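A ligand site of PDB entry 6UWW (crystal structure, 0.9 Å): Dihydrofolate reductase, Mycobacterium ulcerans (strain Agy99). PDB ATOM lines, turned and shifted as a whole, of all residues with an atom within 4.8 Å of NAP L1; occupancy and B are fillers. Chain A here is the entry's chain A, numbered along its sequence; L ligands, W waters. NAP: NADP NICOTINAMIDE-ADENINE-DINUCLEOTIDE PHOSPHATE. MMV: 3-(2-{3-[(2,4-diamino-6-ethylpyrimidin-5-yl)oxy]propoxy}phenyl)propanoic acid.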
ATOM      1  N   ILE A  15      -9.815 -12.672 -22.740  1.00  0.00           N
ATOM      2  CA  ILE A  15      -9.688 -11.976 -21.473  1.00  0.00           C
ATOM      3  C   ILE A  15      -8.820 -12.839 -20.572  1.00  0.00           C
ATOM      4  O   ILE A  15      -9.080 -14.038 -20.458  1.00  0.00           O
ATOM      5  CB  ILE A  15     -11.081 -11.637 -20.854  1.00  0.00           C
ATOM      6  CG1 ILE A  15     -10.945 -10.859 -19.548  1.00  0.00           C
ATOM      7  CG2 ILE A  15     -11.969 -12.861 -20.700  1.00  0.00           C
ATOM      8  CD1 ILE A  15     -12.207 -10.177 -19.121  1.00  0.00           C
ATOM      9  N   TRP A  16      -7.793 -12.252 -19.970  1.00  0.00           N
ATOM     10  CA  TRP A  16      -6.907 -12.977 -19.072  1.00  0.00           C
ATOM     11  C   TRP A  16      -6.288 -12.018 -18.066  1.00  0.00           C
ATOM     12  O   TRP A  16      -6.232 -10.815 -18.298  1.00  0.00           O
ATOM     13  CB  TRP A  16      -5.804 -13.765 -19.799  1.00  0.00           C
ATOM     14  CG  TRP A  16      -4.658 -12.990 -20.395  1.00  0.00           C
ATOM     15  CD1 TRP A  16      -3.502 -12.643 -19.775  1.00  0.00           C
ATOM     16  CD2 TRP A  16      -4.531 -12.542 -21.755  1.00  0.00           C
ATOM     17  NE1 TRP A  16      -2.650 -12.017 -20.661  1.00  0.00           N
ATOM     18  CE2 TRP A  16      -3.256 -11.943 -21.886  1.00  0.00           C
ATOM     19  CE3 TRP A  16      -5.364 -12.608 -22.879  1.00  0.00           C
ATOM     20  CZ2 TRP A  16      -2.811 -11.404 -23.086  1.00  0.00           C
ATOM     21  CZ3 TRP A  16      -4.916 -12.071 -24.070  1.00  0.00           C
ATOM     22  CH2 TRP A  16      -3.654 -11.480 -24.166  1.00  0.00           C
ATOM     23  N   ALA A  17      -5.779 -12.606 -16.983  1.00  0.00           N
ATOM     24  CA  ALA A  17      -4.966 -11.918 -15.998  1.00  0.00           C
ATOM     25  C   ALA A  17      -3.606 -12.605 -15.918  1.00  0.00           C
ATOM     26  O   ALA A  17      -3.531 -13.830 -15.829  1.00  0.00           O
ATOM     27  CB  ALA A  17      -5.650 -11.927 -14.622  1.00  0.00           C
ATOM     28  N   ILE A  24      -0.046 -17.175 -16.016  1.00  0.00           N
ATOM     29  CA  ILE A  24      -1.494 -17.158 -15.795  1.00  0.00           C
ATOM     30  C   ILE A  24      -1.984 -18.272 -14.876  1.00  0.00           C
ATOM     31  O   ILE A  24      -3.060 -18.130 -14.299  1.00  0.00           O
ATOM     32  CB  ILE A  24      -2.316 -17.134 -17.105  1.00  0.00           C
ATOM     33  CG1 ILE A  24      -2.193 -18.468 -17.878  1.00  0.00           C
ATOM     34  CG2 ILE A  24      -1.940 -15.943 -17.958  1.00  0.00           C
ATOM     35  CD1 ILE A  24      -3.218 -18.569 -18.993  1.00  0.00           C
ATOM     36  N   GLY A  25      -1.264 -19.384 -14.778  1.00  0.00           N
ATOM     37  CA  GLY A  25      -1.764 -20.533 -14.037  1.00  0.00           C
ATOM     38  C   GLY A  25      -0.633 -21.347 -13.465  1.00  0.00           C
ATOM     39  O   GLY A  25       0.451 -21.447 -14.045  1.00  0.00           O
ATOM     40  N   ARG A  26      -0.908 -21.959 -12.315  1.00  0.00           N
ATOM     41  CA  ARG A  26       0.051 -22.828 -11.637  1.00  0.00           C
ATOM     42  C   ARG A  26      -0.736 -23.739 -10.725  1.00  0.00           C
ATOM     43  O   ARG A  26      -1.693 -23.293 -10.076  1.00  0.00           O
ATOM     44  CB  ARG A  26       1.040 -21.978 -10.839  1.00  0.00           C
ATOM     45  CG  ARG A  26       2.015 -22.767  -9.996  1.00  0.00           C
ATOM     46  CD  ARG A  26       3.029 -21.864  -9.311  1.00  0.00           C
ATOM     47  NE  ARG A  26       3.863 -21.153 -10.277  1.00  0.00           N
ATOM     48  CZ  ARG A  26       4.758 -20.224  -9.947  1.00  0.00           C
ATOM     49  NH1 ARG A  26       4.910 -19.871  -8.677  1.00  0.00           N
ATOM     50  NH2 ARG A  26       5.481 -19.639 -10.889  1.00  0.00           N
ATOM     51  N   GLY A  28      -2.942 -25.923 -11.121  1.00  0.00           N
ATOM     52  CA  GLY A  28      -4.362 -26.049 -11.387  1.00  0.00           C
ATOM     53  C   GLY A  28      -5.190 -24.869 -10.960  1.00  0.00           C
ATOM     54  O   GLY A  28      -6.419 -24.987 -10.906  1.00  0.00           O
ATOM     55  N   GLY A  29      -4.574 -23.735 -10.653  1.00  0.00           N
ATOM     56  CA  GLY A  29      -5.288 -22.542 -10.280  1.00  0.00           C
ATOM     57  C   GLY A  29      -4.550 -21.307 -10.708  1.00  0.00           C
ATOM     58  O   GLY A  29      -3.673 -21.375 -11.581  1.00  0.00           O
ATOM     59  N   ILE A  30      -4.901 -20.177 -10.119  1.00  0.00           N
ATOM     60  CA  ILE A  30      -4.317 -18.883 -10.419  1.00  0.00           C
ATOM     61  C   ILE A  30      -3.508 -18.462  -9.198  1.00  0.00           C
ATOM     62  O   ILE A  30      -4.061 -18.403  -8.094  1.00  0.00           O
ATOM     63  CB  ILE A  30      -5.396 -17.843 -10.768  1.00  0.00           C
ATOM     64  CG1 ILE A  30      -6.148 -18.279 -12.032  1.00  0.00           C
ATOM     65  CG2 ILE A  30      -4.778 -16.478 -10.931  1.00  0.00           C
ATOM     66  CD1 ILE A  30      -7.327 -17.426 -12.375  1.00  0.00           C
ATOM     67  N   TRP A  32      -2.399 -16.028  -7.404  1.00  0.00           N
ATOM     68  CA  TRP A  32      -2.515 -14.786  -6.646  1.00  0.00           C
ATOM     69  C   TRP A  32      -3.992 -14.580  -6.346  1.00  0.00           C
ATOM     70  O   TRP A  32      -4.861 -15.254  -6.901  1.00  0.00           O
ATOM     71  CB  TRP A  32      -1.964 -13.569  -7.429  1.00  0.00           C
ATOM     72  CG  TRP A  32      -2.650 -13.367  -8.736  1.00  0.00           C
ATOM     73  CD1 TRP A  32      -3.876 -12.795  -8.952  1.00  0.00           C
ATOM     74  CD2 TRP A  32      -2.184 -13.784 -10.022  1.00  0.00           C
ATOM     75  NE1 TRP A  32      -4.202 -12.837 -10.283  1.00  0.00           N
ATOM     76  CE2 TRP A  32      -3.168 -13.434 -10.972  1.00  0.00           C
ATOM     77  CE3 TRP A  32      -1.019 -14.425 -10.472  1.00  0.00           C
ATOM     78  CZ2 TRP A  32      -3.034 -13.715 -12.324  1.00  0.00           C
ATOM     79  CZ3 TRP A  32      -0.894 -14.702 -11.821  1.00  0.00           C
ATOM     80  CH2 TRP A  32      -1.903 -14.343 -12.729  1.00  0.00           C
ATOM     81  N   GLY A  53     -10.972 -23.931 -22.286  1.00  0.00           N
ATOM     82  CA  GLY A  53     -10.471 -25.297 -22.377  1.00  0.00           C
ATOM     83  C   GLY A  53     -10.904 -26.134 -21.201  1.00  0.00           C
ATOM     84  O   GLY A  53     -11.269 -25.640 -20.122  1.00  0.00           O
ATOM     85  N   ARG A  54     -10.831 -27.460 -21.385  1.00  0.00           N
ATOM     86  CA  ARG A  54     -11.318 -28.358 -20.348  1.00  0.00           C
ATOM     87  C   ARG A  54     -10.537 -28.213 -19.048  1.00  0.00           C
ATOM     88  O   ARG A  54     -11.110 -28.368 -17.969  1.00  0.00           O
ATOM     89  CB  ARG A  54     -11.301 -29.792 -20.897  1.00  0.00           C
ATOM     90  CG  ARG A  54     -12.044 -30.824 -20.051  1.00  0.00           C
ATOM     91  CD  ARG A  54     -11.219 -31.443 -18.945  1.00  0.00           C
ATOM     92  NE  ARG A  54      -9.999 -32.015 -19.482  1.00  0.00           N
ATOM     93  CZ  ARG A  54      -8.882 -32.175 -18.795  1.00  0.00           C
ATOM     94  NH1 ARG A  54      -8.827 -31.839 -17.510  1.00  0.00           N
ATOM     95  NH2 ARG A  54      -7.807 -32.652 -19.414  1.00  0.00           N
ATOM     96  N   ARG A  55      -9.218 -27.948 -19.114  1.00  0.00           N
ATOM     97  CA  ARG A  55      -8.476 -27.790 -17.863  1.00  0.00           C
ATOM     98  C   ARG A  55      -8.940 -26.559 -17.096  1.00  0.00           C
ATOM     99  O   ARG A  55      -9.027 -26.585 -15.868  1.00  0.00           O
ATOM    100  CB  ARG A  55      -6.961 -27.793 -18.112  1.00  0.00           C
ATOM    101  CG  ARG A  55      -6.439 -29.136 -18.592  1.00  0.00           C
ATOM    102  CD  ARG A  55      -4.961 -29.099 -18.971  1.00  0.00           C
ATOM    103  NE  ARG A  55      -4.063 -28.560 -17.953  1.00  0.00           N
ATOM    104  CZ  ARG A  55      -3.537 -29.263 -16.947  1.00  0.00           C
ATOM    105  NH1 ARG A  55      -3.836 -30.546 -16.799  1.00  0.00           N
ATOM    106  NH2 ARG A  55      -2.722 -28.678 -16.086  1.00  0.00           N
ATOM    107  N   THR A  56      -9.292 -25.474 -17.801  1.00  0.00           N
ATOM    108  CA  THR A  56      -9.852 -24.309 -17.128  1.00  0.00           C
ATOM    109  C   THR A  56     -11.220 -24.640 -16.524  1.00  0.00           C
ATOM    110  O   THR A  56     -11.513 -24.222 -15.390  1.00  0.00           O
ATOM    111  CB  THR A  56      -9.897 -23.126 -18.089  1.00  0.00           C
ATOM    112  OG1 THR A  56      -8.561 -22.695 -18.356  1.00  0.00           O
ATOM    113  CG2 THR A  56     -10.637 -21.939 -17.494  1.00  0.00           C
ATOM    114  N   SER A  59     -10.605 -26.224 -13.343  1.00  0.00           N
ATOM    115  CA  SER A  59     -10.014 -25.316 -12.373  1.00  0.00           C
ATOM    116  C   SER A  59     -11.031 -24.411 -11.687  1.00  0.00           C
ATOM    117  O   SER A  59     -10.670 -23.733 -10.714  1.00  0.00           O
ATOM    118  CB  SER A  59      -8.950 -24.434 -13.056  1.00  0.00           C
ATOM    119  OG  SER A  59      -9.523 -23.345 -13.778  1.00  0.00           O
ATOM    120  N   VAL A  75     -14.185 -26.719 -24.372  1.00  0.00           N
ATOM    121  CA  VAL A  75     -13.493 -27.324 -25.506  1.00  0.00           C
ATOM    122  C   VAL A  75     -12.675 -28.510 -25.016  1.00  0.00           C
ATOM    123  O   VAL A  75     -11.799 -28.355 -24.141  1.00  0.00           O
ATOM    124  CB  VAL A  75     -12.603 -26.282 -26.192  1.00  0.00           C
ATOM    125  CG1 VAL A  75     -11.908 -26.894 -27.393  1.00  0.00           C
ATOM    126  CG2 VAL A  75     -13.406 -25.053 -26.612  1.00  0.00           C
ATOM    127  N   THR A  76     -12.931 -29.686 -25.576  1.00  0.00           N
ATOM    128  CA  THR A  76     -12.292 -30.940 -25.175  1.00  0.00           C
ATOM    129  C   THR A  76     -12.197 -31.849 -26.381  1.00  0.00           C
ATOM    130  O   THR A  76     -13.005 -31.752 -27.300  1.00  0.00           O
ATOM    131  CB  THR A  76     -13.100 -31.632 -24.061  1.00  0.00           C
ATOM    132  OG1 THR A  76     -12.461 -32.851 -23.673  1.00  0.00           O
ATOM    133  CG2 THR A  76     -14.516 -31.973 -24.490  1.00  0.00           C
ATOM    134  N   ARG A  77     -11.224 -32.758 -26.366  1.00  0.00           N
ATOM    135  CA  ARG A  77     -11.223 -33.853 -27.331  1.00  0.00           C
ATOM    136  C   ARG A  77     -11.951 -35.079 -26.807  1.00  0.00           C
ATOM    137  O   ARG A  77     -12.095 -36.061 -27.548  1.00  0.00           O
ATOM    138  CB  ARG A  77      -9.796 -34.229 -27.722  1.00  0.00           C
ATOM    139  CG  ARG A  77      -9.088 -33.131 -28.476  1.00  0.00           C
ATOM    140  CD  ARG A  77      -7.805 -33.652 -29.063  1.00  0.00           C
ATOM    141  NE  ARG A  77      -7.058 -32.664 -29.825  1.00  0.00           N
ATOM    142  CZ  ARG A  77      -6.214 -31.783 -29.286  1.00  0.00           C
ATOM    143  NH1 ARG A  77      -6.015 -31.763 -27.974  1.00  0.00           N
ATOM    144  NH2 ARG A  77      -5.561 -30.926 -30.062  1.00  0.00           N
ATOM    145  N   GLN A  78     -12.426 -35.050 -25.573  1.00  0.00           N
ATOM    146  CA  GLN A  78     -13.107 -36.194 -24.979  1.00  0.00           C
ATOM    147  C   GLN A  78     -14.558 -36.153 -25.419  1.00  0.00           C
ATOM    148  O   GLN A  78     -15.405 -35.513 -24.788  1.00  0.00           O
ATOM    149  CB  GLN A  78     -13.003 -36.152 -23.471  1.00  0.00           C
ATOM    150  CG  GLN A  78     -11.605 -36.148 -22.981  1.00  0.00           C
ATOM    151  CD  GLN A  78     -11.592 -36.205 -21.491  1.00  0.00           C
ATOM    152  OE1 GLN A  78     -12.025 -37.194 -20.914  1.00  0.00           O
ATOM    153  NE2 GLN A  78     -11.138 -35.150 -20.862  1.00  0.00           N
ATOM    154  N   GLY A  90     -16.021 -29.886 -29.507  1.00  0.00           N
ATOM    155  CA  GLY A  90     -14.822 -30.647 -29.826  1.00  0.00           C
ATOM    156  C   GLY A  90     -13.686 -29.876 -30.441  1.00  0.00           C
ATOM    157  O   GLY A  90     -12.643 -30.477 -30.747  1.00  0.00           O
ATOM    158  N   SER A  91     -13.819 -28.567 -30.620  1.00  0.00           N
ATOM    159  CA  SER A  91     -12.748 -27.726 -31.132  1.00  0.00           C
ATOM    160  C   SER A  91     -13.091 -26.284 -30.792  1.00  0.00           C
ATOM    161  O   SER A  91     -14.237 -25.944 -30.509  1.00  0.00           O
ATOM    162  CB  SER A  91     -12.616 -27.833 -32.655  1.00  0.00           C
ATOM    163  OG  SER A  91     -13.713 -27.214 -33.288  1.00  0.00           O
ATOM    164  N   ILE A 108     -11.861 -17.366 -22.319  1.00  0.00           N
ATOM    165  CA  ILE A 108     -11.485 -17.117 -20.941  1.00  0.00           C
ATOM    166  C   ILE A 108     -10.354 -18.025 -20.457  1.00  0.00           C
ATOM    167  O   ILE A 108     -10.062 -18.033 -19.257  1.00  0.00           O
ATOM    168  CB  ILE A 108     -12.696 -17.185 -19.997  1.00  0.00           C
ATOM    169  CG1 ILE A 108     -13.216 -18.601 -19.855  1.00  0.00           C
ATOM    170  CG2 ILE A 108     -13.772 -16.218 -20.451  1.00  0.00           C
ATOM    171  CD1 ILE A 108     -14.096 -18.802 -18.606  1.00  0.00           C
ATOM    172  N   GLY A 109      -9.716 -18.746 -21.366  1.00  0.00           N
ATOM    173  CA  GLY A 109      -8.511 -19.494 -21.080  1.00  0.00           C
ATOM    174  C   GLY A 109      -8.687 -20.977 -21.333  1.00  0.00           C
ATOM    175  O   GLY A 109      -9.745 -21.427 -21.750  1.00  0.00           O
ATOM    176  N   GLY A 110      -7.627 -21.748 -21.083  1.00  0.00           N
ATOM    177  CA  GLY A 110      -6.346 -21.356 -20.556  1.00  0.00           C
ATOM    178  C   GLY A 110      -5.300 -21.145 -21.628  1.00  0.00           C
ATOM    179  O   GLY A 110      -5.619 -20.679 -22.716  1.00  0.00           O
ATOM    180  N   ALA A 111      -4.039 -21.428 -21.297  1.00  0.00           N
ATOM    181  CA  ALA A 111      -2.948 -21.140 -22.214  1.00  0.00           C
ATOM    182  C   ALA A 111      -3.094 -21.865 -23.546  1.00  0.00           C
ATOM    183  O   ALA A 111      -2.791 -21.298 -24.609  1.00  0.00           O
ATOM    184  CB  ALA A 111      -1.599 -21.474 -21.568  1.00  0.00           C
ATOM    185  N   GLN A 112      -3.521 -23.127 -23.525  1.00  0.00           N
ATOM    186  CA  GLN A 112      -3.645 -23.861 -24.770  1.00  0.00           C
ATOM    187  C   GLN A 112      -4.675 -23.207 -25.673  1.00  0.00           C
ATOM    188  O   GLN A 112      -4.453 -23.027 -26.872  1.00  0.00           O
ATOM    189  CB  GLN A 112      -4.027 -25.323 -24.533  1.00  0.00           C
ATOM    190  CG  GLN A 112      -3.092 -26.086 -23.617  1.00  0.00           C
ATOM    191  CD  GLN A 112      -3.402 -27.557 -23.587  1.00  0.00           C
ATOM    192  OE1 GLN A 112      -4.056 -28.097 -24.510  1.00  0.00           O
ATOM    193  NE2 GLN A 112      -2.975 -28.236 -22.534  1.00  0.00           N
ATOM    194  N   ILE A 113      -5.833 -22.864 -25.094  1.00  0.00           N
ATOM    195  CA  ILE A 113      -6.929 -22.300 -25.881  1.00  0.00           C
ATOM    196  C   ILE A 113      -6.613 -20.876 -26.311  1.00  0.00           C
ATOM    197  O   ILE A 113      -6.950 -20.488 -27.434  1.00  0.00           O
ATOM    198  CB  ILE A 113      -8.275 -22.425 -25.156  1.00  0.00           C
ATOM    199  CG1 ILE A 113      -8.632 -23.878 -24.925  1.00  0.00           C
ATOM    200  CG2 ILE A 113      -9.351 -21.712 -25.955  1.00  0.00           C
ATOM    201  CD1 ILE A 113      -8.577 -24.793 -26.077  1.00  0.00           C
ATOM    202  N   TYR A 114      -5.941 -20.078 -25.470  1.00  0.00           N
ATOM    203  CA  TYR A 114      -5.598 -18.737 -25.909  1.00  0.00           C
ATOM    204  C   TYR A 114      -4.749 -18.778 -27.177  1.00  0.00           C
ATOM    205  O   TYR A 114      -4.895 -17.922 -28.058  1.00  0.00           O
ATOM    206  CB  TYR A 114      -4.833 -17.951 -24.841  1.00  0.00           C
ATOM    207  CG  TYR A 114      -5.619 -17.507 -23.632  1.00  0.00           C
ATOM    208  CD1 TYR A 114      -6.862 -16.911 -23.750  1.00  0.00           C
ATOM    209  CD2 TYR A 114      -5.072 -17.644 -22.361  1.00  0.00           C
ATOM    210  CE1 TYR A 114      -7.549 -16.489 -22.620  1.00  0.00           C
ATOM    211  CE2 TYR A 114      -5.738 -17.221 -21.238  1.00  0.00           C
ATOM    212  CZ  TYR A 114      -6.987 -16.656 -21.362  1.00  0.00           C
ATOM    213  OH  TYR A 114      -7.644 -16.308 -20.217  1.00  0.00           O
ATOM    214  N   LEU A 116      -4.734 -20.886 -29.608  1.00  0.00           N
ATOM    215  CA  LEU A 116      -5.565 -21.165 -30.765  1.00  0.00           C
ATOM    216  C   LEU A 116      -6.504 -20.010 -31.085  1.00  0.00           C
ATOM    217  O   LEU A 116      -6.838 -19.779 -32.248  1.00  0.00           O
ATOM    218  CB  LEU A 116      -6.397 -22.416 -30.506  1.00  0.00           C
ATOM    219  CG  LEU A 116      -5.623 -23.689 -30.185  1.00  0.00           C
ATOM    220  CD1 LEU A 116      -6.597 -24.811 -29.903  1.00  0.00           C
ATOM    221  CD2 LEU A 116      -4.658 -24.030 -31.317  1.00  0.00           C
ATOM    222  N   ALA A 140       1.253 -22.339 -16.719  1.00  0.00           N
ATOM    223  CA  ALA A 140       0.553 -21.880 -17.904  1.00  0.00           C
ATOM    224  C   ALA A 140       0.887 -20.407 -18.102  1.00  0.00           C
ATOM    225  O   ALA A 140       0.823 -19.630 -17.143  1.00  0.00           O
ATOM    226  CB  ALA A 140      -0.961 -22.073 -17.736  1.00  0.00           C
HETATM  227  PA  NAP L   1      -6.705 -25.124 -21.057  1.00  0.00           P
HETATM  228  O1A NAP L   1      -7.726 -24.530 -20.146  1.00  0.00           O
HETATM  229  O2A NAP L   1      -6.268 -24.357 -22.229  1.00  0.00           O
HETATM  230  O5B NAP L   1      -7.325 -26.556 -21.427  1.00  0.00           O
HETATM  231  C5B NAP L   1      -6.588 -27.463 -22.231  1.00  0.00           C
HETATM  232  C4B NAP L   1      -7.546 -28.548 -22.721  1.00  0.00           C
HETATM  233  O4B NAP L   1      -8.305 -28.041 -23.713  1.00  0.00           O
HETATM  234  C3B NAP L   1      -6.828 -29.795 -23.270  1.00  0.00           C
HETATM  235  O3B NAP L   1      -6.324 -30.634 -22.270  1.00  0.00           O
HETATM  236  C2B NAP L   1      -7.999 -30.305 -24.152  1.00  0.00           C
HETATM  237  O2B NAP L   1      -8.999 -30.954 -23.280  1.00  0.00           O
HETATM  238  C1B NAP L   1      -8.573 -29.164 -24.688  1.00  0.00           C
HETATM  239  N9A NAP L   1      -8.027 -28.749 -25.983  1.00  0.00           N
HETATM  240  C8A NAP L   1      -6.871 -28.118 -26.284  1.00  0.00           C
HETATM  241  N7A NAP L   1      -6.737 -28.005 -27.612  1.00  0.00           N
HETATM  242  C5A NAP L   1      -7.837 -28.583 -28.145  1.00  0.00           C
HETATM  243  C6A NAP L   1      -8.248 -28.762 -29.462  1.00  0.00           C
HETATM  244  N6A NAP L   1      -7.545 -28.327 -30.640  1.00  0.00           N
HETATM  245  N1A NAP L   1      -9.391 -29.376 -29.700  1.00  0.00           N
HETATM  246  C2A NAP L   1     -10.163 -29.831 -28.657  1.00  0.00           C
HETATM  247  N3A NAP L   1      -9.811 -29.685 -27.383  1.00  0.00           N
HETATM  248  C4A NAP L   1      -8.631 -29.055 -27.164  1.00  0.00           C
HETATM  249  O3  NAP L   1      -5.445 -25.623 -20.187  1.00  0.00           O
HETATM  250  PN  NAP L   1      -4.129 -24.880 -19.615  1.00  0.00           P
HETATM  251  O1N NAP L   1      -3.359 -24.216 -20.703  1.00  0.00           O
HETATM  252  O2N NAP L   1      -3.420 -25.924 -18.796  1.00  0.00           O
HETATM  253  O5D NAP L   1      -4.722 -23.698 -18.680  1.00  0.00           O
HETATM  254  C5D NAP L   1      -5.259 -23.992 -17.389  1.00  0.00           C
HETATM  255  C4D NAP L   1      -4.503 -23.129 -16.374  1.00  0.00           C
HETATM  256  O4D NAP L   1      -4.662 -21.796 -16.668  1.00  0.00           O
HETATM  257  C3D NAP L   1      -4.971 -23.338 -14.912  1.00  0.00           C
HETATM  258  O3D NAP L   1      -3.904 -23.137 -14.032  1.00  0.00           O
HETATM  259  C2D NAP L   1      -5.964 -22.157 -14.810  1.00  0.00           C
HETATM  260  O2D NAP L   1      -6.171 -21.866 -13.390  1.00  0.00           O
HETATM  261  C1D NAP L   1      -5.344 -21.125 -15.446  1.00  0.00           C
HETATM  262  N1N NAP L   1      -6.135 -20.037 -16.012  1.00  0.00           N
HETATM  263  C2N NAP L   1      -5.766 -18.746 -15.760  1.00  0.00           C
HETATM  264  C3N NAP L   1      -6.481 -17.678 -16.292  1.00  0.00           C
HETATM  265  C7N NAP L   1      -6.068 -16.275 -16.036  1.00  0.00           C
HETATM  266  O7N NAP L   1      -6.575 -15.356 -16.638  1.00  0.00           O
HETATM  267  N7N NAP L   1      -5.094 -16.043 -15.076  1.00  0.00           N
HETATM  268  C4N NAP L   1      -7.556 -17.949 -17.112  1.00  0.00           C
HETATM  269  C5N NAP L   1      -7.931 -19.238 -17.351  1.00  0.00           C
HETATM  270  C6N NAP L   1      -7.217 -20.295 -16.805  1.00  0.00           C
HETATM  271  P2B NAP L   1      -9.008 -32.556 -23.043  1.00  0.00           P
HETATM  272  O1X NAP L   1      -9.080 -33.205 -24.402  1.00  0.00           O
HETATM  273  O2X NAP L   1      -7.720 -32.890 -22.292  1.00  0.00           O
HETATM  274  O3X NAP L   1     -10.254 -32.756 -22.197  1.00  0.00           O
HETATM  275  C1  MMV L   2      -9.805 -14.543 -16.898  1.00  0.00           C
HETATM  276  N2  MMV L   2      -9.585 -13.260 -17.086  1.00  0.00           N
HETATM  277  C3  MMV L   2      -9.420 -12.535 -15.986  1.00  0.00           C
HETATM  278  N4  MMV L   2      -9.459 -13.052 -14.756  1.00  0.00           N
HETATM  279  C5  MMV L   2      -9.716 -14.351 -14.550  1.00  0.00           C
HETATM  280  C6  MMV L   2      -9.903 -15.155 -15.642  1.00  0.00           C
HETATM  281  N7  MMV L   2      -9.973 -15.316 -18.063  1.00  0.00           N
HETATM  282  N8  MMV L   2      -9.183 -11.164 -16.125  1.00  0.00           N
HETATM  283  C9  MMV L   2      -9.790 -14.821 -13.125  1.00  0.00           C
HETATM  284  C10 MMV L   2     -11.065 -14.289 -12.452  1.00  0.00           C
HETATM  285  O11 MMV L   2     -10.128 -16.509 -15.523  1.00  0.00           O
HETATM  286  C12 MMV L   2     -11.497 -16.923 -15.651  1.00  0.00           C
HETATM  287  C13 MMV L   2     -11.562 -18.394 -15.278  1.00  0.00           C
HETATM  288  C14 MMV L   2     -11.274 -18.605 -13.805  1.00  0.00           C
HETATM  289  O15 MMV L   2     -12.313 -17.974 -13.084  1.00  0.00           O
HETATM  290  C16 MMV L   2     -12.225 -17.877 -11.729  1.00  0.00           C
HETATM  291  C17 MMV L   2     -13.237 -17.210 -11.071  1.00  0.00           C
HETATM  292  C18 MMV L   2     -13.163 -17.075  -9.681  1.00  0.00           C
HETATM  293  C19 MMV L   2     -12.086 -17.622  -8.982  1.00  0.00           C
HETATM  294  C20 MMV L   2     -11.088 -18.303  -9.660  1.00  0.00           C
HETATM  295  C21 MMV L   2     -11.143 -18.438 -11.034  1.00  0.00           C
HETATM  296  C22 MMV L   2     -14.381 -16.617 -11.890  1.00  0.00           C
HETATM  297  C23 MMV L   2     -15.718 -16.668 -11.171  1.00  0.00           C
HETATM  298  C24 MMV L   2     -16.848 -15.934 -11.872  1.00  0.00           C
HETATM  299  O25 MMV L   2     -17.981 -16.227 -11.429  1.00  0.00           O
HETATM  300  O26 MMV L   2     -16.643 -15.143 -12.836  1.00  0.00           O
HETATM  301  O   HOH W   1      -3.541 -30.975 -22.139  1.00  0.00           O
HETATM  302  O   HOH W   2      -8.714 -36.014 -24.533  1.00  0.00           O
HETATM  303  O   HOH W   3      -1.916 -25.074 -13.665  1.00  0.00           O
HETATM  304  O   HOH W   4      -1.721 -25.816 -16.747  1.00  0.00           O
HETATM  305  O   HOH W   5      -8.039 -28.874 -33.490  1.00  0.00           O
HETATM  306  O   HOH W   6      -8.641 -20.837 -13.025  1.00  0.00           O
HETATM  307  O   HOH W   7      -4.668 -27.966 -31.462  1.00  0.00           O
HETATM  308  O   HOH W   8      -4.207 -27.425 -28.733  1.00  0.00           O
HETATM  309  O   HOH W   9      -9.546 -26.168 -31.917  1.00  0.00           O
HETATM  310  O   HOH W  10      -0.685 -25.266 -20.878  1.00  0.00           O
HETATM  311  O   HOH W  11      -1.638 -27.567 -20.188  1.00  0.00           O
HETATM  312  O   HOH W  12     -10.142 -30.464 -32.206  1.00  0.00           O
HETATM  313  O   HOH W  13      -5.859 -34.509 -22.215  1.00  0.00           O
HETATM  314  O   HOH W  14      -6.755 -33.359 -25.859  1.00  0.00           O
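OG1 of Thr 76 sits at hydrogen-bond distance from O3X of NAP L1, at 2.7 Å. An oxygen (O1A) of NAP L1 lies within hydrogen-bond range of the backbone NH (N) of Thr 56, 3.0 Å away. An oxygen (O1A) of NAP L1 lies within hydrogen-bond range of the side-chain hydroxyl (OG1) of Thr 56 (2.7 Å). N of Ala 17 is in hydrogen-bond range of O7N of NAP L1 (2.9 Å). A nitrogen (N7N) of NAP L1 sits at hydrogen-bond distance from the backbone carbonyl oxygen (O) of Ala 17 (2.8 Å). O4B of NAP L1 lies within hydrogen-bond range of N of Arg 54 (3.5 Å). NE of Arg 54 is in salt-bridge range of O3X of NAP L1 (2.8 Å). An oxygen (O5B) of NAP L1 is in hydrogen-bond range of the backbone NH (N) of Arg 55 (3.3 Å). An oxygen (O2N) of NAP L1 is in salt-bridge range of the guanidinium group (NE) of Arg 55 (2.8 Å). O3X of NAP L1 sits at hydrogen-bond distance from NE2 of Gln 78. N of Ala 111 is in hydrogen-bond range of O1N of NAP L1 (2.9 Å). The backbone NH (N) of Gly 110 sits at hydrogen-bond distance from an oxygen (O1A) of NAP L1. N of Arg 77 is in hydrogen-bond range of O1X of NAP L1, at 2.9 Å. The backbone carbonyl oxygen (O) of Ile 24 lies within hydrogen-bond range of a nitrogen (N7N) of NAP L1. N of Gly 29 lies within hydrogen-bond range of O3D of NAP L1, 3.5 Å away. O3D of NAP L1 lies within hydrogen-bond range of O of Gly 29 (3.0 Å). O1N of NAP L1 is in hydrogen-bond range of N of Gln 112 (3.0 Å). O2A of NAP L1 is in hydrogen-bond range of N of Ile 113 (3.3 Å). O of Ile 108 lies within hydrogen-bond range of N7 of MMV L2 (3.0 Å). OH of Tyr 114 lies within hydrogen-bond range of N7 of MMV L2, 3.3 Å away. A nitrogen (N7) of MMV L2 lies within hydrogen-bond range of the backbone carbonyl oxygen (O) of Ile 15 (2.9 Å).
The side-chain hydroxyl (OG1) of Thr 76 lies within hydrogen-bond range of the backbone NH (N) of Gln 78 (2.9 Å). The backbone NH (N) of Gly 110 is in hydrogen-bond range of the side-chain hydroxyl (OG1) of Thr 56 (3.0 Å). The backbone carbonyl oxygen (O) of Thr 56 lies within hydrogen-bond range of the side-chain hydroxyl (OG) of Ser 59, 2.7 Å away. The backbone NH (N) of Arg 54 is in hydrogen-bond range of the backbone carbonyl oxygen (O) of Val 75, at 3.1 Å. The backbone NH (N) of Ile 24 lies within hydrogen-bond range of the backbone carbonyl oxygen (O) of Ala 140, 2.8 Å away. The backbone carbonyl oxygen (O) of Ile 108 sits at hydrogen-bond distance from the side-chain hydroxyl (OH) of Tyr 114 (3.1 Å). O of Gly 25 lies within hydrogen-bond range of N of Ala 140, at 2.9 Å. The backbone NH (N) of Gly 53 lies within hydrogen-bond range of the backbone carbonyl oxygen (O) of Gly 109 (2.8 Å).
Merely in contact with NAP L1: Trp 16, Gly 25, Arg 26, Gly 28, Ile 30, Gly 53, Ser 59, Val 75, Gly 90, Ile 108, Gly 109, Tyr 114, Leu 116 and Ala 140. The nearest printed residue that does not touch NAP L1 is Ser 91 (4.01 Å).
Water W4 lies within hydrogen-bond range of an oxygen (O2N) of NAP L1 (2.7 Å) and the guanidinium group (NH2) of Arg 55 (3.1 Å). Water W6 bridges an oxygen (O2D) of NAP L1 (2.7 Å) and the side-chain hydroxyl (OG) of Ser 59 (2.8 Å). Water W14 bridges O1X of NAP L1 (2.7 Å) and NH1 of Arg 77 (2.8 Å). Water W3 lies within hydrogen-bond range of an oxygen (O3D) of NAP L1 and the backbone NH (N) of Gly 28. Water W12 bridges a nitrogen (N1A) of NAP L1 and the backbone carbonyl oxygen of Gly 90. Water W7 lies within hydrogen-bond range of a nitrogen (N6A) of NAP L1 and the guanidinium group of Arg 77.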
